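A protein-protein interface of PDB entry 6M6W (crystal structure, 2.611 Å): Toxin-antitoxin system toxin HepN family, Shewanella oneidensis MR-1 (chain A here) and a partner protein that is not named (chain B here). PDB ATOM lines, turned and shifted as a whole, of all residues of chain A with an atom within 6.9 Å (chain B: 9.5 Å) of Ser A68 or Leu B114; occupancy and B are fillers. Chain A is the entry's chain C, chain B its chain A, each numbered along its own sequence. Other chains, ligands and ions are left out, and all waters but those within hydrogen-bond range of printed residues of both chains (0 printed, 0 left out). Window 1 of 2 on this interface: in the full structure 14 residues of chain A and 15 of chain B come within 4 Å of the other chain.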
ATOM      1  N   ILE A  51     -14.903  -9.246 -21.089  1.00  0.00           N
ATOM      2  CA  ILE A  51     -13.493  -9.306 -20.709  1.00  0.00           C
ATOM      3  C   ILE A  51     -13.287 -10.310 -19.579  1.00  0.00           C
ATOM      4  O   ILE A  51     -12.297 -11.053 -19.562  1.00  0.00           O
ATOM      5  CB  ILE A  51     -12.971  -7.902 -20.343  1.00  0.00           C
ATOM      6  CG1 ILE A  51     -12.976  -7.000 -21.581  1.00  0.00           C
ATOM      7  CG2 ILE A  51     -11.575  -7.976 -19.743  1.00  0.00           C
ATOM      8  CD1 ILE A  51     -12.680  -5.548 -21.280  1.00  0.00           C
ATOM      9  N   ASN A  55     -10.857 -13.376 -19.973  1.00  0.00           N
ATOM     10  CA  ASN A  55      -9.727 -13.574 -19.068  1.00  0.00           C
ATOM     11  C   ASN A  55      -9.855 -14.858 -18.262  1.00  0.00           C
ATOM     12  O   ASN A  55      -8.842 -15.493 -17.951  1.00  0.00           O
ATOM     13  CB  ASN A  55      -9.568 -12.380 -18.129  1.00  0.00           C
ATOM     14  CG  ASN A  55      -8.920 -11.192 -18.804  1.00  0.00           C
ATOM     15  OD1 ASN A  55      -8.173 -11.350 -19.769  1.00  0.00           O
ATOM     16  ND2 ASN A  55      -9.190  -9.996 -18.294  1.00  0.00           N
ATOM     17  N   ILE A  65      -0.624 -13.530 -20.646  1.00  0.00           N
ATOM     18  CA  ILE A  65      -0.887 -12.352 -19.801  1.00  0.00           C
ATOM     19  C   ILE A  65      -1.305 -11.213 -20.694  1.00  0.00           C
ATOM     20  O   ILE A  65      -0.506 -10.740 -21.532  1.00  0.00           O
ATOM     21  CB  ILE A  65       0.352 -12.002 -18.967  1.00  0.00           C
ATOM     22  CG1 ILE A  65       0.985 -13.287 -18.420  1.00  0.00           C
ATOM     23  CG2 ILE A  65      -0.015 -11.058 -17.843  1.00  0.00           C
ATOM     24  CD1 ILE A  65       2.324 -13.087 -17.790  1.00  0.00           C
ATOM     25  N   PRO A  66      -2.533 -10.692 -20.578  1.00  0.00           N
ATOM     26  CA  PRO A  66      -2.954  -9.562 -21.408  1.00  0.00           C
ATOM     27  C   PRO A  66      -2.184  -8.297 -21.052  1.00  0.00           C
ATOM     28  O   PRO A  66      -2.076  -7.924 -19.880  1.00  0.00           O
ATOM     29  CB  PRO A  66      -4.449  -9.418 -21.101  1.00  0.00           C
ATOM     30  CG  PRO A  66      -4.674 -10.164 -19.837  1.00  0.00           C
ATOM     31  CD  PRO A  66      -3.643 -11.247 -19.775  1.00  0.00           C
ATOM     32  N   GLN A  67      -1.637  -7.646 -22.074  1.00  0.00           N
ATOM     33  CA  GLN A  67      -0.944  -6.376 -21.916  1.00  0.00           C
ATOM     34  C   GLN A  67      -1.894  -5.183 -21.927  1.00  0.00           C
ATOM     35  O   GLN A  67      -1.502  -4.089 -21.508  1.00  0.00           O
ATOM     36  CB  GLN A  67       0.142  -6.247 -22.983  1.00  0.00           C
ATOM     37  CG  GLN A  67       1.038  -7.471 -23.007  1.00  0.00           C
ATOM     38  CD  GLN A  67       1.849  -7.595 -21.731  1.00  0.00           C
ATOM     39  OE1 GLN A  67       2.684  -6.747 -21.425  1.00  0.00           O
ATOM     40  NE2 GLN A  67       1.580  -8.647 -20.960  1.00  0.00           N
ATOM     41  N   SER A  68      -3.123  -5.373 -22.406  1.00  0.00           N
ATOM     42  CA  SER A  68      -4.157  -4.349 -22.394  1.00  0.00           C
ATOM     43  C   SER A  68      -5.500  -5.067 -22.341  1.00  0.00           C
ATOM     44  O   SER A  68      -5.579  -6.284 -22.524  1.00  0.00           O
ATOM     45  CB  SER A  68      -4.071  -3.418 -23.610  1.00  0.00           C
ATOM     46  OG  SER A  68      -4.255  -4.121 -24.825  1.00  0.00           O
ATOM     47  N   SER A  69      -6.562  -4.305 -22.071  1.00  0.00           N
ATOM     48  CA  SER A  69      -7.895  -4.899 -22.006  1.00  0.00           C
ATOM     49  C   SER A  69      -8.287  -5.537 -23.333  1.00  0.00           C
ATOM     50  O   SER A  69      -8.794  -6.666 -23.366  1.00  0.00           O
ATOM     51  CB  SER A  69      -8.922  -3.849 -21.578  1.00  0.00           C
ATOM     52  OG  SER A  69      -8.719  -3.457 -20.228  1.00  0.00           O
ATOM     53  N   ARG A  70      -8.051  -4.830 -24.441  1.00  0.00           N
ATOM     54  CA  ARG A  70      -8.410  -5.357 -25.753  1.00  0.00           C
ATOM     55  C   ARG A  70      -7.702  -6.673 -26.067  1.00  0.00           C
ATOM     56  O   ARG A  70      -8.202  -7.448 -26.889  1.00  0.00           O
ATOM     57  CB  ARG A  70      -8.100  -4.320 -26.838  1.00  0.00           C
ATOM     58  CG  ARG A  70      -6.634  -4.274 -27.236  1.00  0.00           C
ATOM     59  CD  ARG A  70      -6.282  -3.010 -27.994  1.00  0.00           C
ATOM     60  NE  ARG A  70      -4.850  -2.930 -28.266  1.00  0.00           N
ATOM     61  CZ  ARG A  70      -4.031  -2.052 -27.698  1.00  0.00           C
ATOM     62  NH1 ARG A  70      -2.741  -2.047 -28.003  1.00  0.00           N
ATOM     63  NH2 ARG A  70      -4.505  -1.175 -26.823  1.00  0.00           N
ATOM     64  N   ASP A  71      -6.568  -6.956 -25.409  1.00  0.00           N
ATOM     65  CA  ASP A  71      -5.756  -8.141 -25.710  1.00  0.00           C
ATOM     66  C   ASP A  71      -6.418  -9.410 -25.176  1.00  0.00           C
ATOM     67  O   ASP A  71      -6.181 -10.492 -25.729  1.00  0.00           O
ATOM     68  CB  ASP A  71      -4.337  -7.932 -25.124  1.00  0.00           C
ATOM     69  CG  ASP A  71      -3.348  -9.117 -25.341  1.00  0.00           C
ATOM     70  OD1 ASP A  71      -3.676 -10.178 -25.935  1.00  0.00           O
ATOM     71  OD2 ASP A  71      -2.171  -8.969 -24.945  1.00  0.00           O
ATOM     72  N   SER A  72      -7.311  -9.291 -24.179  1.00  0.00           N
ATOM     73  CA  SER A  72      -7.999 -10.471 -23.665  1.00  0.00           C
ATOM     74  C   SER A  72      -8.711 -11.208 -24.793  1.00  0.00           C
ATOM     75  O   SER A  72      -8.763 -12.443 -24.814  1.00  0.00           O
ATOM     76  CB  SER A  72      -8.979 -10.062 -22.571  1.00  0.00           C
ATOM     77  OG  SER A  72      -8.311  -9.674 -21.377  1.00  0.00           O
ATOM     78  N   PHE A  73      -9.260 -10.461 -25.748  1.00  0.00           N
ATOM     79  CA  PHE A  73      -9.892 -11.066 -26.909  1.00  0.00           C
ATOM     80  C   PHE A  73      -8.870 -11.525 -27.945  1.00  0.00           C
ATOM     81  O   PHE A  73      -9.132 -12.487 -28.674  1.00  0.00           O
ATOM     82  CB  PHE A  73     -10.888 -10.076 -27.503  1.00  0.00           C
ATOM     83  CG  PHE A  73     -11.976  -9.702 -26.547  1.00  0.00           C
ATOM     84  CD1 PHE A  73     -12.908 -10.642 -26.142  1.00  0.00           C
ATOM     85  CD2 PHE A  73     -12.023  -8.435 -25.992  1.00  0.00           C
ATOM     86  CE1 PHE A  73     -13.902 -10.310 -25.241  1.00  0.00           C
ATOM     87  CE2 PHE A  73     -13.011  -8.097 -25.087  1.00  0.00           C
ATOM     88  CZ  PHE A  73     -13.950  -9.037 -24.712  1.00  0.00           C
ATOM     89  N   VAL A  94     -14.384  -2.638 -26.724  1.00  0.00           N
ATOM     90  CA  VAL A  94     -13.531  -2.250 -25.605  1.00  0.00           C
ATOM     91  C   VAL A  94     -13.037  -0.819 -25.773  1.00  0.00           C
ATOM     92  O   VAL A  94     -13.035  -0.032 -24.819  1.00  0.00           O
ATOM     93  CB  VAL A  94     -12.358  -3.236 -25.458  1.00  0.00           C
ATOM     94  CG1 VAL A  94     -11.350  -2.709 -24.449  1.00  0.00           C
ATOM     95  CG2 VAL A  94     -12.870  -4.606 -25.052  1.00  0.00           C
ATOM     96  N   ARG A  97     -15.756   1.471 -24.762  1.00  0.00           N
ATOM     97  CA  ARG A  97     -15.804   1.527 -23.307  1.00  0.00           C
ATOM     98  C   ARG A  97     -14.689   2.420 -22.787  1.00  0.00           C
ATOM     99  O   ARG A  97     -14.924   3.318 -21.973  1.00  0.00           O
ATOM    100  CB  ARG A  97     -15.697   0.130 -22.705  1.00  0.00           C
ATOM    101  CG  ARG A  97     -15.632   0.164 -21.182  1.00  0.00           C
ATOM    102  CD  ARG A  97     -14.805  -0.954 -20.572  1.00  0.00           C
ATOM    103  NE  ARG A  97     -13.395  -0.871 -20.934  1.00  0.00           N
ATOM    104  CZ  ARG A  97     -12.451  -1.661 -20.430  1.00  0.00           C
ATOM    105  NH1 ARG A  97     -12.768  -2.582 -19.530  1.00  0.00           N
ATOM    106  NH2 ARG A  97     -11.189  -1.521 -20.812  1.00  0.00           N
ATOM    107  N   SER B  77      -0.526   2.859 -30.572  1.00  0.00           N
ATOM    108  CA  SER B  77      -0.888   1.464 -30.782  1.00  0.00           C
ATOM    109  C   SER B  77      -0.176   0.522 -29.820  1.00  0.00           C
ATOM    110  O   SER B  77      -0.313  -0.700 -29.954  1.00  0.00           O
ATOM    111  CB  SER B  77      -0.591   1.040 -32.226  1.00  0.00           C
ATOM    112  OG  SER B  77       0.803   1.054 -32.486  1.00  0.00           O
ATOM    113  N   ALA B  78       0.567   1.049 -28.851  1.00  0.00           N
ATOM    114  CA  ALA B  78       1.276   0.196 -27.915  1.00  0.00           C
ATOM    115  C   ALA B  78       0.349  -0.271 -26.798  1.00  0.00           C
ATOM    116  O   ALA B  78      -0.689   0.336 -26.516  1.00  0.00           O
ATOM    117  CB  ALA B  78       2.479   0.925 -27.321  1.00  0.00           C
ATOM    118  N   SER B  79       0.746  -1.366 -26.158  1.00  0.00           N
ATOM    119  CA  SER B  79      -0.047  -1.936 -25.082  1.00  0.00           C
ATOM    120  C   SER B  79      -0.137  -0.967 -23.905  1.00  0.00           C
ATOM    121  O   SER B  79       0.659  -0.035 -23.764  1.00  0.00           O
ATOM    122  CB  SER B  79       0.561  -3.257 -24.620  1.00  0.00           C
ATOM    123  OG  SER B  79       1.775  -3.038 -23.921  1.00  0.00           O
ATOM    124  N   THR B  80      -1.133  -1.202 -23.049  1.00  0.00           N
ATOM    125  CA  THR B  80      -1.251  -0.429 -21.817  1.00  0.00           C
ATOM    126  C   THR B  80      -0.057  -0.667 -20.906  1.00  0.00           C
ATOM    127  O   THR B  80       0.456   0.274 -20.285  1.00  0.00           O
ATOM    128  CB  THR B  80      -2.548  -0.783 -21.092  1.00  0.00           C
ATOM    129  OG1 THR B  80      -3.665  -0.438 -21.920  1.00  0.00           O
ATOM    130  CG2 THR B  80      -2.644  -0.025 -19.780  1.00  0.00           C
ATOM    131  N   VAL B  81       0.384  -1.925 -20.800  1.00  0.00           N
ATOM    132  CA  VAL B  81       1.528  -2.251 -19.954  1.00  0.00           C
ATOM    133  C   VAL B  81       2.750  -1.422 -20.346  1.00  0.00           C
ATOM    134  O   VAL B  81       3.445  -0.874 -19.483  1.00  0.00           O
ATOM    135  CB  VAL B  81       1.818  -3.762 -20.017  1.00  0.00           C
ATOM    136  CG1 VAL B  81       3.260  -4.048 -19.628  1.00  0.00           C
ATOM    137  CG2 VAL B  81       0.855  -4.530 -19.122  1.00  0.00           C
ATOM    138  N   LEU B  82       3.022  -1.296 -21.646  1.00  0.00           N
ATOM    139  CA  LEU B  82       4.226  -0.587 -22.069  1.00  0.00           C
ATOM    140  C   LEU B  82       4.015   0.926 -22.109  1.00  0.00           C
ATOM    141  O   LEU B  82       4.977   1.685 -21.914  1.00  0.00           O
ATOM    142  CB  LEU B  82       4.695  -1.108 -23.427  1.00  0.00           C
ATOM    143  CG  LEU B  82       5.800  -0.318 -24.148  1.00  0.00           C
ATOM    144  CD1 LEU B  82       7.111  -0.535 -23.435  1.00  0.00           C
ATOM    145  CD2 LEU B  82       5.929  -0.778 -25.579  1.00  0.00           C
ATOM    146  N   CYS B  83       2.779   1.393 -22.339  1.00  0.00           N
ATOM    147  CA  CYS B  83       2.495   2.808 -22.123  1.00  0.00           C
ATOM    148  C   CYS B  83       2.728   3.189 -20.668  1.00  0.00           C
ATOM    149  O   CYS B  83       3.245   4.274 -20.378  1.00  0.00           O
ATOM    150  CB  CYS B  83       1.064   3.143 -22.548  1.00  0.00           C
ATOM    151  SG  CYS B  83       0.752   3.179 -24.333  1.00  0.00           S
ATOM    152  N   GLN B  84       2.351   2.308 -19.735  1.00  0.00           N
ATOM    153  CA  GLN B  84       2.590   2.583 -18.323  1.00  0.00           C
ATOM    154  C   GLN B  84       4.080   2.706 -18.034  1.00  0.00           C
ATOM    155  O   GLN B  84       4.499   3.558 -17.241  1.00  0.00           O
ATOM    156  CB  GLN B  84       1.960   1.490 -17.459  1.00  0.00           C
ATOM    157  CG  GLN B  84       2.344   1.570 -15.988  1.00  0.00           C
ATOM    158  CD  GLN B  84       1.611   2.670 -15.242  1.00  0.00           C
ATOM    159  OE1 GLN B  84       0.924   3.498 -15.839  1.00  0.00           O
ATOM    160  NE2 GLN B  84       1.770   2.691 -13.924  1.00  0.00           N
ATOM    161  N   LYS B 106      -4.409   9.404 -18.901  1.00  0.00           N
ATOM    162  CA  LYS B 106      -5.077   8.348 -19.649  1.00  0.00           C
ATOM    163  C   LYS B 106      -4.370   7.008 -19.473  1.00  0.00           C
ATOM    164  O   LYS B 106      -5.009   5.977 -19.228  1.00  0.00           O
ATOM    165  CB  LYS B 106      -5.160   8.737 -21.121  1.00  0.00           C
ATOM    166  CG  LYS B 106      -5.783   7.707 -22.017  1.00  0.00           C
ATOM    167  CD  LYS B 106      -5.664   8.155 -23.449  1.00  0.00           C
ATOM    168  CE  LYS B 106      -6.154   7.088 -24.388  1.00  0.00           C
ATOM    169  NZ  LYS B 106      -7.602   7.326 -24.646  1.00  0.00           N
ATOM    170  N   THR B 107      -3.040   7.010 -19.576  1.00  0.00           N
ATOM    171  CA  THR B 107      -2.269   5.782 -19.418  1.00  0.00           C
ATOM    172  C   THR B 107      -2.457   5.194 -18.027  1.00  0.00           C
ATOM    173  O   THR B 107      -2.828   4.024 -17.877  1.00  0.00           O
ATOM    174  CB  THR B 107      -0.790   6.062 -19.677  1.00  0.00           C
ATOM    175  OG1 THR B 107      -0.619   6.572 -21.000  1.00  0.00           O
ATOM    176  CG2 THR B 107       0.024   4.806 -19.511  1.00  0.00           C
ATOM    177  N   ILE B 108      -2.197   6.000 -16.995  1.00  0.00           N
ATOM    178  CA  ILE B 108      -2.217   5.503 -15.624  1.00  0.00           C
ATOM    179  C   ILE B 108      -3.596   4.968 -15.260  1.00  0.00           C
ATOM    180  O   ILE B 108      -3.717   3.917 -14.624  1.00  0.00           O
ATOM    181  CB  ILE B 108      -1.756   6.615 -14.667  1.00  0.00           C
ATOM    182  CG1 ILE B 108      -0.256   6.865 -14.850  1.00  0.00           C
ATOM    183  CG2 ILE B 108      -2.085   6.271 -13.224  1.00  0.00           C
ATOM    184  CD1 ILE B 108       0.245   8.118 -14.178  1.00  0.00           C
ATOM    185  N   SER B 109      -4.656   5.648 -15.702  1.00  0.00           N
ATOM    186  CA  SER B 109      -6.009   5.177 -15.414  1.00  0.00           C
ATOM    187  C   SER B 109      -6.281   3.835 -16.080  1.00  0.00           C
ATOM    188  O   SER B 109      -6.745   2.889 -15.432  1.00  0.00           O
ATOM    189  CB  SER B 109      -7.038   6.215 -15.858  1.00  0.00           C
ATOM    190  OG  SER B 109      -8.346   5.667 -15.833  1.00  0.00           O
ATOM    191  N   MET B 110      -6.017   3.743 -17.388  1.00  0.00           N
ATOM    192  CA  MET B 110      -6.232   2.492 -18.109  1.00  0.00           C
ATOM    193  C   MET B 110      -5.458   1.345 -17.477  1.00  0.00           C
ATOM    194  O   MET B 110      -5.914   0.197 -17.504  1.00  0.00           O
ATOM    195  CB  MET B 110      -5.825   2.649 -19.575  1.00  0.00           C
ATOM    196  CG  MET B 110      -6.745   3.533 -20.393  1.00  0.00           C
ATOM    197  SD  MET B 110      -6.237   3.615 -22.117  1.00  0.00           S
ATOM    198  CE  MET B 110      -6.684   1.967 -22.660  1.00  0.00           C
ATOM    199  N   TYR B 111      -4.287   1.635 -16.908  1.00  0.00           N
ATOM    200  CA  TYR B 111      -3.463   0.577 -16.335  1.00  0.00           C
ATOM    201  C   TYR B 111      -4.054   0.053 -15.033  1.00  0.00           C
ATOM    202  O   TYR B 111      -4.037  -1.158 -14.785  1.00  0.00           O
ATOM    203  CB  TYR B 111      -2.038   1.083 -16.122  1.00  0.00           C
ATOM    204  CG  TYR B 111      -1.090   0.019 -15.635  1.00  0.00           C
ATOM    205  CD1 TYR B 111      -0.466  -0.839 -16.531  1.00  0.00           C
ATOM    206  CD2 TYR B 111      -0.812  -0.127 -14.285  1.00  0.00           C
ATOM    207  CE1 TYR B 111       0.405  -1.819 -16.092  1.00  0.00           C
ATOM    208  CE2 TYR B 111       0.058  -1.099 -13.836  1.00  0.00           C
ATOM    209  CZ  TYR B 111       0.664  -1.942 -14.742  1.00  0.00           C
ATOM    210  OH  TYR B 111       1.531  -2.913 -14.297  1.00  0.00           O
ATOM    211  N   GLN B 112      -4.576   0.943 -14.186  1.00  0.00           N
ATOM    212  CA  GLN B 112      -5.221   0.491 -12.957  1.00  0.00           C
ATOM    213  C   GLN B 112      -6.475  -0.316 -13.265  1.00  0.00           C
ATOM    214  O   GLN B 112      -6.795  -1.274 -12.550  1.00  0.00           O
ATOM    215  CB  GLN B 112      -5.555   1.686 -12.062  1.00  0.00           C
ATOM    216  CG  GLN B 112      -4.471   2.745 -12.009  1.00  0.00           C
ATOM    217  CD  GLN B 112      -4.832   3.928 -11.131  1.00  0.00           C
ATOM    218  OE1 GLN B 112      -5.906   4.515 -11.270  1.00  0.00           O
ATOM    219  NE2 GLN B 112      -3.933   4.285 -10.223  1.00  0.00           N
ATOM    220  N   HIS B 113      -7.184   0.040 -14.338  1.00  0.00           N
ATOM    221  CA  HIS B 113      -8.316  -0.770 -14.773  1.00  0.00           C
ATOM    222  C   HIS B 113      -7.852  -2.128 -15.279  1.00  0.00           C
ATOM    223  O   HIS B 113      -8.498  -3.150 -15.017  1.00  0.00           O
ATOM    224  CB  HIS B 113      -9.110  -0.040 -15.855  1.00  0.00           C
ATOM    225  CG  HIS B 113     -10.031   1.010 -15.323  1.00  0.00           C
ATOM    226  ND1 HIS B 113      -9.590   2.253 -14.923  1.00  0.00           N
ATOM    227  CD2 HIS B 113     -11.368   0.999 -15.109  1.00  0.00           C
ATOM    228  CE1 HIS B 113     -10.616   2.966 -14.496  1.00  0.00           C
ATOM    229  NE2 HIS B 113     -11.707   2.228 -14.597  1.00  0.00           N
ATOM    230  N   LEU B 114      -6.735  -2.161 -16.009  1.00  0.00           N
ATOM    231  CA  LEU B 114      -6.257  -3.429 -16.544  1.00  0.00           C
ATOM    232  C   LEU B 114      -5.749  -4.336 -15.432  1.00  0.00           C
ATOM    233  O   LEU B 114      -5.905  -5.559 -15.506  1.00  0.00           O
ATOM    234  CB  LEU B 114      -5.157  -3.186 -17.580  1.00  0.00           C
ATOM    235  CG  LEU B 114      -4.340  -4.422 -17.963  1.00  0.00           C
ATOM    236  CD1 LEU B 114      -5.205  -5.334 -18.827  1.00  0.00           C
ATOM    237  CD2 LEU B 114      -3.043  -4.063 -18.670  1.00  0.00           C
ATOM    238  N   GLN B 115      -5.169  -3.753 -14.379  1.00  0.00           N
ATOM    239  CA  GLN B 115      -4.686  -4.557 -13.263  1.00  0.00           C
ATOM    240  C   GLN B 115      -5.841  -5.245 -12.549  1.00  0.00           C
ATOM    241  O   GLN B 115      -5.722  -6.402 -12.130  1.00  0.00           O
ATOM    242  CB  GLN B 115      -3.897  -3.680 -12.288  1.00  0.00           C
ATOM    243  CG  GLN B 115      -2.521  -3.259 -12.786  1.00  0.00           C
ATOM    244  CD  GLN B 115      -1.548  -4.420 -12.920  1.00  0.00           C
ATOM    245  OE1 GLN B 115      -1.647  -5.230 -13.842  1.00  0.00           O
ATOM    246  NE2 GLN B 115      -0.597  -4.503 -11.996  1.00  0.00           N
ATOM    247  N   ALA B 116      -6.966  -4.541 -12.400  1.00  0.00           N
ATOM    248  CA  ALA B 116      -8.164  -5.159 -11.842  1.00  0.00           C
ATOM    249  C   ALA B 116      -8.647  -6.318 -12.705  1.00  0.00           C
ATOM    250  O   ALA B 116      -9.036  -7.368 -12.180  1.00  0.00           O
ATOM    251  CB  ALA B 116      -9.265  -4.113 -11.681  1.00  0.00           C
ATOM    252  N   GLU B 117      -8.643  -6.146 -14.031  1.00  0.00           N
ATOM    253  CA  GLU B 117      -9.172  -7.198 -14.895  1.00  0.00           C
ATOM    254  C   GLU B 117      -8.304  -8.451 -14.858  1.00  0.00           C
ATOM    255  O   GLU B 117      -8.830  -9.571 -14.874  1.00  0.00           O
ATOM    256  CB  GLU B 117      -9.309  -6.716 -16.342  1.00  0.00           C
ATOM    257  CG  GLU B 117     -10.210  -5.521 -16.582  1.00  0.00           C
ATOM    258  CD  GLU B 117     -10.091  -5.007 -18.009  1.00  0.00           C
ATOM    259  OE1 GLU B 117     -10.956  -4.218 -18.443  1.00  0.00           O
ATOM    260  OE2 GLU B 117      -9.137  -5.413 -18.707  1.00  0.00           O
ATOM    261  N   ARG B 118      -6.981  -8.293 -14.821  1.00  0.00           N
ATOM    262  CA  ARG B 118      -6.072  -9.401 -15.080  1.00  0.00           C
ATOM    263  C   ARG B 118      -5.312  -9.898 -13.854  1.00  0.00           C
ATOM    264  O   ARG B 118      -4.456 -10.774 -14.007  1.00  0.00           O
ATOM    265  CB  ARG B 118      -5.056  -9.007 -16.159  1.00  0.00           C
ATOM    266  CG  ARG B 118      -3.995  -8.057 -15.636  1.00  0.00           C
ATOM    267  CD  ARG B 118      -2.982  -7.668 -16.690  1.00  0.00           C
ATOM    268  NE  ARG B 118      -1.943  -6.826 -16.104  1.00  0.00           N
ATOM    269  CZ  ARG B 118      -0.698  -6.737 -16.556  1.00  0.00           C
ATOM    270  NH1 ARG B 118      -0.315  -7.446 -17.610  1.00  0.00           N
ATOM    271  NH2 ARG B 118       0.168  -5.942 -15.946  1.00  0.00           N
ATOM    272  N   GLN B 119      -5.588  -9.377 -12.651  1.00  0.00           N
ATOM    273  CA  GLN B 119      -4.770  -9.753 -11.496  1.00  0.00           C
ATOM    274  C   GLN B 119      -4.850 -11.249 -11.223  1.00  0.00           C
ATOM    275  O   GLN B 119      -3.845 -11.876 -10.868  1.00  0.00           O
ATOM    276  CB  GLN B 119      -5.165  -8.964 -10.247  1.00  0.00           C
ATOM    277  CG  GLN B 119      -4.290  -9.339  -9.044  1.00  0.00           C
ATOM    278  CD  GLN B 119      -3.868  -8.152  -8.196  1.00  0.00           C
ATOM    279  OE1 GLN B 119      -4.413  -7.916  -7.117  1.00  0.00           O
ATOM    280  NE2 GLN B 119      -2.875  -7.406  -8.676  1.00  0.00           N
ATOM    281  N   ALA B 120      -6.039 -11.835 -11.366  1.00  0.00           N
ATOM    282  CA  ALA B 120      -6.169 -13.274 -11.170  1.00  0.00           C
ATOM    283  C   ALA B 120      -5.240 -14.039 -12.107  1.00  0.00           C
ATOM    284  O   ALA B 120      -4.704 -15.092 -11.741  1.00  0.00           O
ATOM    285  CB  ALA B 120      -7.619 -13.704 -11.385  1.00  0.00           C
ATOM    286  N   ILE B 121      -5.035 -13.524 -13.320  1.00  0.00           N
ATOM    287  CA  ILE B 121      -4.116 -14.165 -14.256  1.00  0.00           C
ATOM    288  C   ILE B 121      -2.670 -14.036 -13.784  1.00  0.00           C
ATOM    289  O   ILE B 121      -1.924 -15.023 -13.764  1.00  0.00           O
ATOM    290  CB  ILE B 121      -4.308 -13.601 -15.676  1.00  0.00           C
ATOM    291  CG1 ILE B 121      -5.590 -14.167 -16.291  1.00  0.00           C
ATOM    292  CG2 ILE B 121      -3.101 -13.903 -16.546  1.00  0.00           C
ATOM    293  CD1 ILE B 121      -5.871 -13.673 -17.690  1.00  0.00           C
ATOM    294  N   ILE B 122      -2.240 -12.827 -13.404  1.00  0.00           N
ATOM    295  CA  ILE B 122      -0.858 -12.670 -12.952  1.00  0.00           C
ATOM    296  C   ILE B 122      -0.612 -13.485 -11.686  1.00  0.00           C
ATOM    297  O   ILE B 122       0.461 -14.077 -11.515  1.00  0.00           O
ATOM    298  CB  ILE B 122      -0.475 -11.180 -12.793  1.00  0.00           C
ATOM    299  CG1 ILE B 122      -1.016 -10.558 -11.506  1.00  0.00           C
ATOM    300  CG2 ILE B 122      -0.919 -10.383 -14.015  1.00  0.00           C
ATOM    301  CD1 ILE B 122      -0.419  -9.191 -11.206  1.00  0.00           C
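Ile A51 touches Glu B117.
Asn A55 touches Ile B121.
CG2 of Ile A65 touches NH1 of Arg B118 (3.6 Å).
Ile A65 touches Ile B122.
CD1 of Ile B121 touches CD of Pro A66, at 3.9 Å.
Gln A67 touches Leu B114 (O to CD2, 3.2 Å).
Thr B80 touches Ser A68 (OG1 to CB, 3.4 Å).
C of Ser A68 touches CD1 of Leu B114 (3.5 Å).
Ser A69 touches Leu B114 (N to CD1, 3.7 Å).
Arg A70 touches Ser B79 (NH1 to CA, 3.98 Å).
Of the 25 printed residues of chain B, 10 touch a printed residue of chain A.
The side-chain hydroxyl (OG) of Ser B79 is in hydrogen-bond range of the backbone NH (N) of Leu B82 (3.1 Å).
The backbone carbonyl oxygen of Ser B79 lies within hydrogen-bond range of the side-chain sulfur of Cys B83, at 3.3 Å.
The side-chain amide oxygen of Gln B115 is in hydrogen-bond range of the guanidinium group of Arg B118 (2.8 Å).
ND2 of Asn A55 sits close to OG of Ser A72 (3.2 Å).
The backbone NH (N) of Gln A67 is in hydrogen-bond range of the side-chain carboxylate (OD2) of Asp A71 (3.2 Å).
NH2 of Arg A97 sits at hydrogen-bond distance from OG of Ser A69.
The backbone carbonyl oxygen of Ser B77 is in hydrogen-bond range of the guanidinium group of Arg A70 (3.4 Å).
The backbone carbonyl oxygen of Ala B78 lies within hydrogen-bond range of the guanidinium group of Arg A70 (3.5 Å).
N of Thr B80 lies within hydrogen-bond range of O of Gln A67, 3.3 Å away.
O of Gln A67 sits at hydrogen-bond distance from N of Val B81, at 3.0 Å.
ND2 of Asn A55 is in hydrogen-bond range of O of Glu B117.
The side-chain carboxylate (OE2) of Glu B117 sits at hydrogen-bond distance from the side-chain hydroxyl (OG) of Ser A69 (2.5 Å).
The side-chain carboxylate of Glu B117 is in salt-bridge range of the guanidinium group of Arg A97 (2.7 Å).
The backbone carbonyl oxygen of Pro A66 sits at hydrogen-bond distance from the guanidinium group of Arg B118, at 2.9 Å.
Ser A68 touches two residues of chain B.
Of the printed residues of chain A, Ser B79 touches Gln A67 (3.4 Å) and Arg A70 (3.98 Å).
Of the printed residues of chain A, Arg B118 touches Ile A65 and Pro A66.
Printed residues of chain B within 4 Å of Ile A65: Arg B118 and Ile B122.
Of the printed residues of chain A, Ser B77 touches Arg A70.
Printed residues of chain A within 4 Å of Thr B80: Gln A67 (3.3 Å) and Ser A68 (3.4 Å).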
